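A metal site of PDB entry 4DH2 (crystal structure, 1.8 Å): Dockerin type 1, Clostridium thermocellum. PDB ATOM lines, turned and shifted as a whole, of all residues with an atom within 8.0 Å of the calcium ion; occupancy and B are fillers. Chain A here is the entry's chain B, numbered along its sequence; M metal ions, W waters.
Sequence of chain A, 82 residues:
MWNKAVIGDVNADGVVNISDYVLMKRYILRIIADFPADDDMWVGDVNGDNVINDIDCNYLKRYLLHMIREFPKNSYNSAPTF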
ATOM      1  N   MET A  24      -9.734  19.334 -14.258  1.00  0.00           N
ATOM      2  CA  MET A  24      -9.076  20.524 -13.751  1.00  0.00           C
ATOM      3  C   MET A  24      -9.991  21.759 -13.893  1.00  0.00           C
ATOM      4  O   MET A  24     -10.154  22.542 -12.952  1.00  0.00           O
ATOM      5  CB  MET A  24      -7.787  20.763 -14.527  1.00  0.00           C
ATOM      6  CG  MET A  24      -7.124  22.077 -14.220  1.00  0.00           C
ATOM      7  SD  MET A  24      -6.355  22.097 -12.612  1.00  0.00           S
ATOM      8  CE  MET A  24      -4.804  21.338 -13.130  1.00  0.00           C
ATOM      9  N   MET A  41      -2.654  18.761  -4.547  1.00  0.00           N
ATOM     10  CA  MET A  41      -1.563  19.663  -4.834  1.00  0.00           C
ATOM     11  C   MET A  41      -0.465  18.946  -5.619  1.00  0.00           C
ATOM     12  O   MET A  41       0.120  19.517  -6.537  1.00  0.00           O
ATOM     13  CB  MET A  41      -1.027  20.255  -3.529  1.00  0.00           C
ATOM     14  CG  MET A  41      -0.137  21.447  -3.738  1.00  0.00           C
ATOM     15  SD  MET A  41      -0.927  22.944  -4.426  1.00  0.00           S
ATOM     16  CE  MET A  41      -1.966  23.423  -3.049  1.00  0.00           C
ATOM     17  N   GLY A  44      -2.213  18.348  -9.129  1.00  0.00           N
ATOM     18  CA  GLY A  44      -2.826  19.493  -9.791  1.00  0.00           C
ATOM     19  C   GLY A  44      -1.975  20.718  -9.938  1.00  0.00           C
ATOM     20  O   GLY A  44      -2.255  21.544 -10.804  1.00  0.00           O
ATOM     21  N   ASP A  45      -0.963  20.889  -9.065  1.00  0.00           N
ATOM     22  CA  ASP A  45      -0.083  22.040  -9.162  1.00  0.00           C
ATOM     23  C   ASP A  45       1.075  21.650 -10.059  1.00  0.00           C
ATOM     24  O   ASP A  45       2.103  21.151  -9.577  1.00  0.00           O
ATOM     25  CB  ASP A  45       0.464  22.437  -7.788  1.00  0.00           C
ATOM     26  CG  ASP A  45       1.564  23.481  -7.873  1.00  0.00           C
ATOM     27  OD1 ASP A  45       1.558  24.261  -8.829  1.00  0.00           O
ATOM     28  OD2 ASP A  45       2.447  23.511  -6.977  1.00  0.00           O
ATOM     29  N   VAL A  46       0.913  21.850 -11.365  1.00  0.00           N
ATOM     30  CA  VAL A  46       1.869  21.292 -12.319  1.00  0.00           C
ATOM     31  C   VAL A  46       3.075  22.197 -12.552  1.00  0.00           C
ATOM     32  O   VAL A  46       4.095  21.729 -13.072  1.00  0.00           O
ATOM     33  CB  VAL A  46       1.216  20.979 -13.671  1.00  0.00           C
ATOM     34  CG1 VAL A  46       0.075  20.016 -13.507  1.00  0.00           C
ATOM     35  CG2 VAL A  46       0.733  22.253 -14.350  1.00  0.00           C
ATOM     36  N   ASN A  47       2.973  23.468 -12.197  1.00  0.00           N
ATOM     37  CA  ASN A  47       4.109  24.387 -12.334  1.00  0.00           C
ATOM     38  C   ASN A  47       4.864  24.549 -11.029  1.00  0.00           C
ATOM     39  O   ASN A  47       5.924  25.169 -10.992  1.00  0.00           O
ATOM     40  CB  ASN A  47       3.704  25.747 -12.912  1.00  0.00           C
ATOM     41  CG  ASN A  47       2.851  26.558 -11.975  1.00  0.00           C
ATOM     42  OD1 ASN A  47       2.128  26.001 -11.181  1.00  0.00           O
ATOM     43  ND2 ASN A  47       2.907  27.876 -12.081  1.00  0.00           N
ATOM     44  N   GLY A  48       4.314  23.989  -9.955  1.00  0.00           N
ATOM     45  CA  GLY A  48       5.004  23.915  -8.686  1.00  0.00           C
ATOM     46  C   GLY A  48       5.107  25.230  -7.935  1.00  0.00           C
ATOM     47  O   GLY A  48       6.082  25.461  -7.237  1.00  0.00           O
ATOM     48  N   ASP A  49       4.095  26.093  -8.060  1.00  0.00           N
ATOM     49  CA  ASP A  49       4.047  27.325  -7.288  1.00  0.00           C
ATOM     50  C   ASP A  49       3.191  27.164  -6.032  1.00  0.00           C
ATOM     51  O   ASP A  49       2.893  28.137  -5.343  1.00  0.00           O
ATOM     52  CB  ASP A  49       3.559  28.510  -8.128  1.00  0.00           C
ATOM     53  CG  ASP A  49       2.178  28.289  -8.707  1.00  0.00           C
ATOM     54  OD1 ASP A  49       1.580  27.238  -8.445  1.00  0.00           O
ATOM     55  OD2 ASP A  49       1.693  29.187  -9.437  1.00  0.00           O
ATOM     56  N   ASN A  50       2.841  25.908  -5.737  1.00  0.00           N
ATOM     57  CA  ASN A  50       2.032  25.563  -4.575  1.00  0.00           C
ATOM     58  C   ASN A  50       0.646  26.192  -4.570  1.00  0.00           C
ATOM     59  O   ASN A  50       0.024  26.397  -3.525  1.00  0.00           O
ATOM     60  CB  ASN A  50       2.758  25.919  -3.286  1.00  0.00           C
ATOM     61  CG  ASN A  50       2.707  24.803  -2.286  1.00  0.00           C
ATOM     62  OD1 ASN A  50       2.719  23.622  -2.659  1.00  0.00           O
ATOM     63  ND2 ASN A  50       2.626  25.157  -1.013  1.00  0.00           N
ATOM     64  N   VAL A  51       0.158  26.473  -5.769  1.00  0.00           N
ATOM     65  CA  VAL A  51      -1.219  26.931  -5.964  1.00  0.00           C
ATOM     66  C   VAL A  51      -1.815  26.050  -7.079  1.00  0.00           C
ATOM     67  O   VAL A  51      -1.077  25.629  -7.969  1.00  0.00           O
ATOM     68  CB  VAL A  51      -1.248  28.371  -6.406  1.00  0.00           C
ATOM     69  CG1 VAL A  51      -2.670  28.816  -6.631  1.00  0.00           C
ATOM     70  CG2 VAL A  51      -0.585  29.266  -5.344  1.00  0.00           C
ATOM     71  N   ILE A  52      -3.101  25.749  -6.987  1.00  0.00           N
ATOM     72  CA  ILE A  52      -3.817  25.153  -8.137  1.00  0.00           C
ATOM     73  C   ILE A  52      -4.764  26.202  -8.659  1.00  0.00           C
ATOM     74  O   ILE A  52      -5.652  26.687  -7.950  1.00  0.00           O
ATOM     75  CB  ILE A  52      -4.655  23.932  -7.764  1.00  0.00           C
ATOM     76  CG1 ILE A  52      -3.821  22.875  -7.052  1.00  0.00           C
ATOM     77  CG2 ILE A  52      -5.264  23.320  -9.039  1.00  0.00           C
ATOM     78  CD1 ILE A  52      -4.674  21.670  -6.546  1.00  0.00           C
ATOM     79  N   ASN A  53      -4.568  26.585  -9.923  1.00  0.00           N
ATOM     80  CA  ASN A  53      -5.452  27.586 -10.510  1.00  0.00           C
ATOM     81  C   ASN A  53      -5.351  27.562 -12.035  1.00  0.00           C
ATOM     82  O   ASN A  53      -4.866  26.586 -12.592  1.00  0.00           O
ATOM     83  CB  ASN A  53      -5.177  28.967  -9.945  1.00  0.00           C
ATOM     84  CG  ASN A  53      -3.810  29.483 -10.251  1.00  0.00           C
ATOM     85  OD1 ASN A  53      -3.063  28.937 -11.090  1.00  0.00           O
ATOM     86  ND2 ASN A  53      -3.445  30.554  -9.567  1.00  0.00           N
ATOM     87  N   ASP A  54      -5.830  28.610 -12.688  1.00  0.00           N
ATOM     88  CA  ASP A  54      -5.958  28.572 -14.132  1.00  0.00           C
ATOM     89  C   ASP A  54      -4.581  28.490 -14.824  1.00  0.00           C
ATOM     90  O   ASP A  54      -4.469  28.048 -15.977  1.00  0.00           O
ATOM     91  CB  ASP A  54      -6.869  29.716 -14.616  1.00  0.00           C
ATOM     92  CG  ASP A  54      -8.378  29.385 -14.393  1.00  0.00           C
ATOM     93  OD1 ASP A  54      -8.832  28.269 -14.792  1.00  0.00           O
ATOM     94  OD2 ASP A  54      -9.118  30.203 -13.775  1.00  0.00           O
ATOM     95  N   ILE A  55      -3.512  28.871 -14.138  1.00  0.00           N
ATOM     96  CA  ILE A  55      -2.186  28.688 -14.701  1.00  0.00           C
ATOM     97  C   ILE A  55      -1.880  27.204 -14.934  1.00  0.00           C
ATOM     98  O   ILE A  55      -1.304  26.811 -15.945  1.00  0.00           O
ATOM     99  CB  ILE A  55      -1.120  29.290 -13.796  1.00  0.00           C
ATOM    100  CG1 ILE A  55      -1.312  30.809 -13.733  1.00  0.00           C
ATOM    101  CG2 ILE A  55       0.290  28.928 -14.310  1.00  0.00           C
ATOM    102  CD1 ILE A  55      -0.507  31.496 -12.617  1.00  0.00           C
ATOM    103  N   ASP A  56      -2.288  26.374 -13.978  1.00  0.00           N
ATOM    104  CA  ASP A  56      -2.123  24.936 -14.110  1.00  0.00           C
ATOM    105  C   ASP A  56      -2.982  24.400 -15.230  1.00  0.00           C
ATOM    106  O   ASP A  56      -2.520  23.560 -16.017  1.00  0.00           O
ATOM    107  CB  ASP A  56      -2.505  24.249 -12.812  1.00  0.00           C
ATOM    108  CG  ASP A  56      -1.618  24.708 -11.697  1.00  0.00           C
ATOM    109  OD1 ASP A  56      -0.435  24.362 -11.734  1.00  0.00           O
ATOM    110  OD2 ASP A  56      -2.095  25.460 -10.825  1.00  0.00           O
ATOM    111  N   CYS A  57      -4.208  24.898 -15.323  1.00  0.00           N
ATOM    112  CA  CYS A  57      -5.088  24.493 -16.429  1.00  0.00           C
ATOM    113  C   CYS A  57      -4.444  24.829 -17.768  1.00  0.00           C
ATOM    114  O   CYS A  57      -4.467  24.038 -18.707  1.00  0.00           O
ATOM    115  CB  CYS A  57      -6.417  25.212 -16.323  1.00  0.00           C
ATOM    116  SG  CYS A  57      -7.755  24.255 -17.048  1.00  0.00           S
ATOM    117  N   TYR A  59      -1.270  25.105 -18.394  1.00  0.00           N
ATOM    118  CA  TYR A  59      -0.158  24.211 -18.645  1.00  0.00           C
ATOM    119  C   TYR A  59      -0.682  22.901 -19.173  1.00  0.00           C
ATOM    120  O   TYR A  59      -0.072  22.299 -20.054  1.00  0.00           O
ATOM    121  CB  TYR A  59       0.694  23.940 -17.402  1.00  0.00           C
ATOM    122  CG  TYR A  59       1.817  24.928 -17.238  1.00  0.00           C
ATOM    123  CD1 TYR A  59       1.716  25.967 -16.327  1.00  0.00           C
ATOM    124  CD2 TYR A  59       2.949  24.837 -18.008  1.00  0.00           C
ATOM    125  CE1 TYR A  59       2.733  26.890 -16.185  1.00  0.00           C
ATOM    126  CE2 TYR A  59       3.973  25.748 -17.891  1.00  0.00           C
ATOM    127  CZ  TYR A  59       3.873  26.771 -16.964  1.00  0.00           C
ATOM    128  OH  TYR A  59       4.899  27.673 -16.851  1.00  0.00           O
ATOM    129  N   LYS A  73       7.084  21.308 -12.888  1.00  0.00           N
ATOM    130  CA  LYS A  73       7.380  20.538 -11.691  1.00  0.00           C
ATOM    131  C   LYS A  73       7.718  19.089 -12.037  1.00  0.00           C
ATOM    132  O   LYS A  73       7.068  18.506 -12.911  1.00  0.00           O
ATOM    133  CB  LYS A  73       6.187  20.587 -10.750  1.00  0.00           C
ATOM    134  CG  LYS A  73       6.369  19.798  -9.462  1.00  0.00           C
ATOM    135  CD  LYS A  73       5.203  20.031  -8.495  1.00  0.00           C
ATOM    136  CE  LYS A  73       4.111  18.972  -8.681  1.00  0.00           C
ATOM    137  NZ  LYS A  73       2.917  19.202  -7.792  1.00  0.00           N
HETATM  138 CA    CA M   1       0.203  25.895  -9.867  1.00  0.00          CA
HETATM  139  O   HOH W   1      -0.428  28.024 -10.484  1.00  0.00           O
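OD1 of Asp 56 lies close to N of Val 46.
The side-chain carboxylate of Asp 45 is in hydrogen-bond range of the backbone NH of Asn 50.
The backbone NH (N) of Asn 53 sits close to the side-chain carboxylate (OD2) of Asp 56, 2.9 Å away.
The side-chain carboxylate (OD1) of Asp 45 lies close to the backbone NH (N) of Gly 48 (3.0 Å).
O of Asp 45 is in hydrogen-bond range of NZ of Lys 73.
Water W1 bridges OD2 of Asp 49 and OD1 of Asn 53.
The nearest printed residue that does not touch the calcium ion is Val 46 (4.4 Å).
O of Val 51 binds the calcium ion (2.3 Å).
The calcium ion is bound by water W1, 2.3 Å away.
The side-chain amide oxygen (OD1) of Asn 47 is bound to the calcium ion, at 2.3 Å.
OD1 of Asp 45 is bound to the calcium ion (2.4 Å).
The calcium ion is bound by OD1 of Asp 49 (2.4 Å).
The calcium ion is bound by OD1 of Asp 56 (2.5 Å).
The side-chain carboxylate (OD2) of Asp 56 binds the calcium ion (2.5 Å).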
